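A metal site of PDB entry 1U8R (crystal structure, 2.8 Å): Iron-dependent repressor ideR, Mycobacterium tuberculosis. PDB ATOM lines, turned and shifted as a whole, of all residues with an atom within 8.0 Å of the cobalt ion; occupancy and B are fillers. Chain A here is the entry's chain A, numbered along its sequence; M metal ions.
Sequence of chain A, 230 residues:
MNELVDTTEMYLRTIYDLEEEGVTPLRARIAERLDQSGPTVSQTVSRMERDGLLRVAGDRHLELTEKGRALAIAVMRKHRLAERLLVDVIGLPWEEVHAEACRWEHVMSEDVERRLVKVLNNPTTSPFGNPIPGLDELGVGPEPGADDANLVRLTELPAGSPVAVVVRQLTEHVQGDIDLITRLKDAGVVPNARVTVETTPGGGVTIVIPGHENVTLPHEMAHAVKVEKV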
ATOM      1  N   GLU A   3      28.666   9.189   8.879  1.00  0.00           N
ATOM      2  CA  GLU A   3      28.039   8.757   7.631  1.00  0.00           C
ATOM      3  C   GLU A   3      26.872   7.803   7.904  1.00  0.00           C
ATOM      4  O   GLU A   3      25.726   8.094   7.570  1.00  0.00           O
ATOM      5  CB  GLU A   3      29.078   8.045   6.752  1.00  0.00           C
ATOM      6  CG  GLU A   3      28.556   7.562   5.399  1.00  0.00           C
ATOM      7  CD  GLU A   3      28.298   8.697   4.437  1.00  0.00           C
ATOM      8  OE1 GLU A   3      29.274   9.344   3.996  1.00  0.00           O
ATOM      9  OE2 GLU A   3      27.117   8.940   4.096  1.00  0.00           O
ATOM     10  N   LEU A   4      27.189   6.681   8.527  1.00  0.00           N
ATOM     11  CA  LEU A   4      26.218   5.650   8.854  1.00  0.00           C
ATOM     12  C   LEU A   4      25.287   5.977  10.042  1.00  0.00           C
ATOM     13  O   LEU A   4      24.302   5.258  10.284  1.00  0.00           O
ATOM     14  CB  LEU A   4      26.979   4.369   9.182  1.00  0.00           C
ATOM     15  CG  LEU A   4      28.020   3.901   8.180  1.00  0.00           C
ATOM     16  CD1 LEU A   4      29.018   3.008   8.886  1.00  0.00           C
ATOM     17  CD2 LEU A   4      27.353   3.146   7.061  1.00  0.00           C
ATOM     18  N   VAL A   5      25.598   7.051  10.752  1.00  0.00           N
ATOM     19  CA  VAL A   5      24.832   7.450  11.932  1.00  0.00           C
ATOM     20  C   VAL A   5      25.201   6.527  13.093  1.00  0.00           C
ATOM     21  O   VAL A   5      25.570   6.981  14.175  1.00  0.00           O
ATOM     22  CB  VAL A   5      23.327   7.342  11.702  1.00  0.00           C
ATOM     23  CG1 VAL A   5      22.597   7.735  12.960  1.00  0.00           C
ATOM     24  CG2 VAL A   5      22.909   8.212  10.543  1.00  0.00           C
ATOM     25  N   ASP A   6      25.083   5.218  12.858  1.00  0.00           N
ATOM     26  CA  ASP A   6      25.438   4.200  13.854  1.00  0.00           C
ATOM     27  C   ASP A   6      26.111   3.031  13.148  1.00  0.00           C
ATOM     28  O   ASP A   6      25.457   2.229  12.478  1.00  0.00           O
ATOM     29  CB  ASP A   6      24.191   3.729  14.594  1.00  0.00           C
ATOM     30  CG  ASP A   6      24.527   2.754  15.703  1.00  0.00           C
ATOM     31  OD1 ASP A   6      23.650   2.508  16.561  1.00  0.00           O
ATOM     32  OD2 ASP A   6      25.659   2.219  15.709  1.00  0.00           O
ATOM     33  N   THR A   7      27.423   2.920  13.297  1.00  0.00           N
ATOM     34  CA  THR A   7      28.165   1.865  12.636  1.00  0.00           C
ATOM     35  C   THR A   7      27.632   0.484  12.959  1.00  0.00           C
ATOM     36  O   THR A   7      27.113  -0.209  12.089  1.00  0.00           O
ATOM     37  CB  THR A   7      29.686   1.953  12.973  1.00  0.00           C
ATOM     38  OG1 THR A   7      30.172   3.269  12.684  1.00  0.00           O
ATOM     39  CG2 THR A   7      30.502   0.937  12.154  1.00  0.00           C
ATOM     40  N   GLU A   9      24.897  -0.798  14.237  1.00  0.00           N
ATOM     41  CA  GLU A   9      23.589  -1.113  13.663  1.00  0.00           C
ATOM     42  C   GLU A   9      23.686  -1.379  12.167  1.00  0.00           C
ATOM     43  O   GLU A   9      23.139  -2.354  11.695  1.00  0.00           O
ATOM     44  CB  GLU A   9      22.601   0.017  13.942  1.00  0.00           C
ATOM     45  CG  GLU A   9      21.676  -0.289  15.093  1.00  0.00           C
ATOM     46  CD  GLU A   9      20.937   0.936  15.585  1.00  0.00           C
ATOM     47  OE1 GLU A   9      20.475   1.752  14.753  1.00  0.00           O
ATOM     48  OE2 GLU A   9      20.791   1.089  16.810  1.00  0.00           O
ATOM     49  N   MET A  10      24.397  -0.526  11.419  1.00  0.00           N
ATOM     50  CA  MET A  10      24.500  -0.738   9.979  1.00  0.00           C
ATOM     51  C   MET A  10      25.236  -2.044   9.619  1.00  0.00           C
ATOM     52  O   MET A  10      24.937  -2.670   8.592  1.00  0.00           O
ATOM     53  CB  MET A  10      25.176   0.467   9.313  1.00  0.00           C
ATOM     54  CG  MET A  10      24.259   1.679   9.139  1.00  0.00           C
ATOM     55  SD  MET A  10      22.638   1.293   8.403  1.00  0.00           S
ATOM     56  CE  MET A  10      23.098   0.520   6.917  1.00  0.00           C
ATOM     57  N   TYR A  11      26.183  -2.455  10.452  1.00  0.00           N
ATOM     58  CA  TYR A  11      26.894  -3.705  10.204  1.00  0.00           C
ATOM     59  C   TYR A  11      25.905  -4.857  10.423  1.00  0.00           C
ATOM     60  O   TYR A  11      25.822  -5.792   9.615  1.00  0.00           O
ATOM     61  CB  TYR A  11      28.105  -3.848  11.125  1.00  0.00           C
ATOM     62  CG  TYR A  11      29.404  -3.293  10.583  1.00  0.00           C
ATOM     63  CD1 TYR A  11      29.510  -1.956  10.196  1.00  0.00           C
ATOM     64  CD2 TYR A  11      30.543  -4.094  10.478  1.00  0.00           C
ATOM     65  CE1 TYR A  11      30.727  -1.430   9.722  1.00  0.00           C
ATOM     66  CE2 TYR A  11      31.757  -3.586  10.001  1.00  0.00           C
ATOM     67  CZ  TYR A  11      31.843  -2.255   9.635  1.00  0.00           C
ATOM     68  OH  TYR A  11      33.025  -1.742   9.191  1.00  0.00           O
ATOM     69  N   ARG A  13      22.529  -4.779  10.307  1.00  0.00           N
ATOM     70  CA  ARG A  13      21.517  -4.772   9.254  1.00  0.00           C
ATOM     71  C   ARG A  13      22.085  -5.254   7.918  1.00  0.00           C
ATOM     72  O   ARG A  13      21.367  -5.887   7.133  1.00  0.00           O
ATOM     73  CB  ARG A  13      20.903  -3.374   9.100  1.00  0.00           C
ATOM     74  CG  ARG A  13      19.415  -3.410   8.815  1.00  0.00           C
ATOM     75  CD  ARG A  13      19.119  -3.021   7.390  1.00  0.00           C
ATOM     76  NE  ARG A  13      19.269  -1.596   7.190  1.00  0.00           N
ATOM     77  CZ  ARG A  13      19.639  -1.000   6.067  1.00  0.00           C
ATOM     78  NH1 ARG A  13      19.927  -1.697   4.978  1.00  0.00           N
ATOM     79  NH2 ARG A  13      19.710   0.330   6.039  1.00  0.00           N
ATOM     80  N   THR A  14      23.351  -4.971   7.654  1.00  0.00           N
ATOM     81  CA  THR A  14      23.922  -5.444   6.399  1.00  0.00           C
ATOM     82  C   THR A  14      24.043  -6.967   6.434  1.00  0.00           C
ATOM     83  O   THR A  14      23.840  -7.644   5.415  1.00  0.00           O
ATOM     84  CB  THR A  14      25.295  -4.810   6.135  1.00  0.00           C
ATOM     85  OG1 THR A  14      25.152  -3.385   6.071  1.00  0.00           O
ATOM     86  CG2 THR A  14      25.854  -5.303   4.802  1.00  0.00           C
ATOM     87  N   LEU A  34      29.348  -0.918   2.564  1.00  0.00           N
ATOM     88  CA  LEU A  34      29.434   0.269   3.383  1.00  0.00           C
ATOM     89  C   LEU A  34      30.598   1.149   2.952  1.00  0.00           C
ATOM     90  O   LEU A  34      30.872   2.172   3.568  1.00  0.00           O
ATOM     91  CB  LEU A  34      29.559  -0.100   4.855  1.00  0.00           C
ATOM     92  CG  LEU A  34      28.403  -0.915   5.423  1.00  0.00           C
ATOM     93  CD1 LEU A  34      28.607  -1.017   6.935  1.00  0.00           C
ATOM     94  CD2 LEU A  34      27.060  -0.265   5.118  1.00  0.00           C
ATOM     95  N   VAL A  75      16.212  -2.961  14.064  1.00  0.00           N
ATOM     96  CA  VAL A  75      16.552  -1.923  13.113  1.00  0.00           C
ATOM     97  C   VAL A  75      15.756  -2.075  11.847  1.00  0.00           C
ATOM     98  O   VAL A  75      15.064  -1.161  11.435  1.00  0.00           O
ATOM     99  CB  VAL A  75      17.998  -1.954  12.737  1.00  0.00           C
ATOM    100  CG1 VAL A  75      18.308  -0.818  11.727  1.00  0.00           C
ATOM    101  CG2 VAL A  75      18.817  -1.832  13.988  1.00  0.00           C
ATOM    102  N   HIS A  79      13.253   0.670  10.098  1.00  0.00           N
ATOM    103  CA  HIS A  79      13.543   1.057   8.736  1.00  0.00           C
ATOM    104  C   HIS A  79      12.298   0.975   7.885  1.00  0.00           C
ATOM    105  O   HIS A  79      11.859   1.972   7.334  1.00  0.00           O
ATOM    106  CB  HIS A  79      14.624   0.152   8.131  1.00  0.00           C
ATOM    107  CG  HIS A  79      14.886   0.440   6.683  1.00  0.00           C
ATOM    108  ND1 HIS A  79      15.556   1.565   6.249  1.00  0.00           N
ATOM    109  CD2 HIS A  79      14.536  -0.236   5.565  1.00  0.00           C
ATOM    110  CE1 HIS A  79      15.602   1.567   4.922  1.00  0.00           C
ATOM    111  NE2 HIS A  79      14.990   0.489   4.487  1.00  0.00           N
ATOM    112  N   HIS A  98      13.944   5.223   0.831  1.00  0.00           N
ATOM    113  CA  HIS A  98      14.929   4.313   1.365  1.00  0.00           C
ATOM    114  C   HIS A  98      16.082   5.063   2.005  1.00  0.00           C
ATOM    115  O   HIS A  98      16.373   4.846   3.178  1.00  0.00           O
ATOM    116  CB  HIS A  98      15.463   3.384   0.289  1.00  0.00           C
ATOM    117  CG  HIS A  98      16.576   2.511   0.777  1.00  0.00           C
ATOM    118  ND1 HIS A  98      16.413   1.617   1.818  1.00  0.00           N
ATOM    119  CD2 HIS A  98      17.880   2.460   0.434  1.00  0.00           C
ATOM    120  CE1 HIS A  98      17.578   1.056   2.095  1.00  0.00           C
ATOM    121  NE2 HIS A  98      18.488   1.546   1.269  1.00  0.00           N
ATOM    122  N   ALA A  99      16.746   5.941   1.253  1.00  0.00           N
ATOM    123  CA  ALA A  99      17.887   6.682   1.784  1.00  0.00           C
ATOM    124  C   ALA A  99      17.573   7.482   3.059  1.00  0.00           C
ATOM    125  O   ALA A  99      18.440   7.685   3.925  1.00  0.00           O
ATOM    126  CB  ALA A  99      18.424   7.611   0.727  1.00  0.00           C
ATOM    127  N   GLU A 100      16.330   7.956   3.160  1.00  0.00           N
ATOM    128  CA  GLU A 100      15.877   8.733   4.297  1.00  0.00           C
ATOM    129  C   GLU A 100      15.718   7.801   5.485  1.00  0.00           C
ATOM    130  O   GLU A 100      16.136   8.102   6.597  1.00  0.00           O
ATOM    131  CB  GLU A 100      14.552   9.372   3.969  1.00  0.00           C
ATOM    132  CG  GLU A 100      14.018  10.322   5.023  1.00  0.00           C
ATOM    133  CD  GLU A 100      14.861  11.562   5.143  1.00  0.00           C
ATOM    134  OE1 GLU A 100      15.460  11.968   4.117  1.00  0.00           O
ATOM    135  OE2 GLU A 100      14.916  12.112   6.260  1.00  0.00           O
ATOM    136  N   ALA A 101      15.095   6.653   5.233  1.00  0.00           N
ATOM    137  CA  ALA A 101      14.856   5.669   6.268  1.00  0.00           C
ATOM    138  C   ALA A 101      16.157   5.065   6.800  1.00  0.00           C
ATOM    139  O   ALA A 101      16.240   4.683   7.961  1.00  0.00           O
ATOM    140  CB  ALA A 101      13.965   4.557   5.737  1.00  0.00           C
ATOM    141  N   CYS A 102      17.166   4.987   5.932  1.00  0.00           N
ATOM    142  CA  CYS A 102      18.455   4.422   6.306  1.00  0.00           C
ATOM    143  C   CYS A 102      19.071   5.211   7.444  1.00  0.00           C
ATOM    144  O   CYS A 102      19.981   4.736   8.127  1.00  0.00           O
ATOM    145  CB  CYS A 102      19.397   4.419   5.116  1.00  0.00           C
ATOM    146  SG  CYS A 102      20.477   3.010   5.024  1.00  0.00           S
ATOM    147  N   ARG A 103      18.581   6.439   7.645  1.00  0.00           N
ATOM    148  CA  ARG A 103      19.076   7.291   8.716  1.00  0.00           C
ATOM    149  C   ARG A 103      18.116   7.290   9.874  1.00  0.00           C
ATOM    150  O   ARG A 103      18.532   7.243  11.020  1.00  0.00           O
ATOM    151  CB  ARG A 103      19.263   8.726   8.244  1.00  0.00           C
ATOM    152  CG  ARG A 103      20.560   8.989   7.537  1.00  0.00           C
ATOM    153  CD  ARG A 103      20.794  10.485   7.438  1.00  0.00           C
ATOM    154  NE  ARG A 103      19.649  11.192   6.840  1.00  0.00           N
ATOM    155  CZ  ARG A 103      19.300  11.075   5.559  1.00  0.00           C
ATOM    156  NH1 ARG A 103      18.248  11.736   5.086  1.00  0.00           N
ATOM    157  NH2 ARG A 103      20.010  10.301   4.754  1.00  0.00           N
ATOM    158  N   TRP A 104      16.820   7.370   9.580  1.00  0.00           N
ATOM    159  CA  TRP A 104      15.794   7.390  10.631  1.00  0.00           C
ATOM    160  C   TRP A 104      15.783   6.110  11.444  1.00  0.00           C
ATOM    161  O   TRP A 104      15.428   6.117  12.620  1.00  0.00           O
ATOM    162  CB  TRP A 104      14.389   7.542  10.027  1.00  0.00           C
ATOM    163  CG  TRP A 104      14.089   8.853   9.424  1.00  0.00           C
ATOM    164  CD1 TRP A 104      14.921   9.629   8.685  1.00  0.00           C
ATOM    165  CD2 TRP A 104      12.824   9.517   9.431  1.00  0.00           C
ATOM    166  NE1 TRP A 104      14.261  10.738   8.213  1.00  0.00           N
ATOM    167  CE2 TRP A 104      12.963  10.688   8.667  1.00  0.00           C
ATOM    168  CE3 TRP A 104      11.588   9.220  10.006  1.00  0.00           C
ATOM    169  CZ2 TRP A 104      11.909  11.571   8.459  1.00  0.00           C
ATOM    170  CZ3 TRP A 104      10.548  10.101   9.797  1.00  0.00           C
ATOM    171  CH2 TRP A 104      10.707  11.258   9.032  1.00  0.00           C
ATOM    172  N   GLU A 105      16.156   5.015  10.794  1.00  0.00           N
ATOM    173  CA  GLU A 105      16.171   3.704  11.421  1.00  0.00           C
ATOM    174  C   GLU A 105      17.025   3.645  12.662  1.00  0.00           C
ATOM    175  O   GLU A 105      16.843   2.775  13.500  1.00  0.00           O
ATOM    176  CB  GLU A 105      16.651   2.674  10.428  1.00  0.00           C
ATOM    177  CG  GLU A 105      18.138   2.711  10.218  1.00  0.00           C
ATOM    178  CD  GLU A 105      18.529   1.850   9.067  1.00  0.00           C
ATOM    179  OE1 GLU A 105      17.663   1.042   8.642  1.00  0.00           O
ATOM    180  OE2 GLU A 105      19.689   1.976   8.589  1.00  0.00           O
ATOM    181  N   HIS A 106      17.954   4.589  12.785  1.00  0.00           N
ATOM    182  CA  HIS A 106      18.857   4.612  13.925  1.00  0.00           C
ATOM    183  C   HIS A 106      18.421   5.578  15.011  1.00  0.00           C
ATOM    184  O   HIS A 106      19.153   5.768  15.961  1.00  0.00           O
ATOM    185  CB  HIS A 106      20.268   4.954  13.468  1.00  0.00           C
ATOM    186  CG  HIS A 106      20.701   4.206  12.246  1.00  0.00           C
ATOM    187  ND1 HIS A 106      21.045   2.876  12.280  1.00  0.00           N
ATOM    188  CD2 HIS A 106      20.767   4.584  10.943  1.00  0.00           C
ATOM    189  CE1 HIS A 106      21.303   2.461  11.049  1.00  0.00           C
ATOM    190  NE2 HIS A 106      21.137   3.472  10.219  1.00  0.00           N
HETATM  191 CO    CO M   1      21.263   2.987   8.167  1.00  0.00          CO
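The cobalt ion is bound by OE2 of Glu 105, at 1.9 Å.
The cobalt ion is bound by NE2 of His 106 (2.1 Å).
The cobalt ion is bound by the backbone carbonyl oxygen (O) of Cys 102 (2.2 Å).
The cobalt ion is bound by the side-chain sulfur (SD) of Met 10 (2.2 Å).
A ring nitrogen (ND1) of His 106 lies within hydrogen-bond range of the side-chain carboxylate of Glu 9, at 2.8 Å.
OE1 of Glu 105 sits close to ND1 of His 79 (3.2 Å).
The side-chain hydroxyl of Thr 14 is in hydrogen-bond range of the backbone carbonyl oxygen of Met 10 (2.6 Å).
The guanidinium group (NH2) of Arg 13 is in salt-bridge range of the side-chain carboxylate (OE1) of Glu 105 (3.4 Å).
SG of Cys 102 lies within hydrogen-bond range of NH2 of Arg 13, at 3.0 Å.
Residues that only touch the cobalt ion: Arg 13.
Five residues have an atom within 4 Å of the cobalt ion: Met 10, Arg 13, Cys 102, Glu 105 and His 106.
The nearest printed residue that does not touch the cobalt ion is Leu 4 (4.3 Å).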
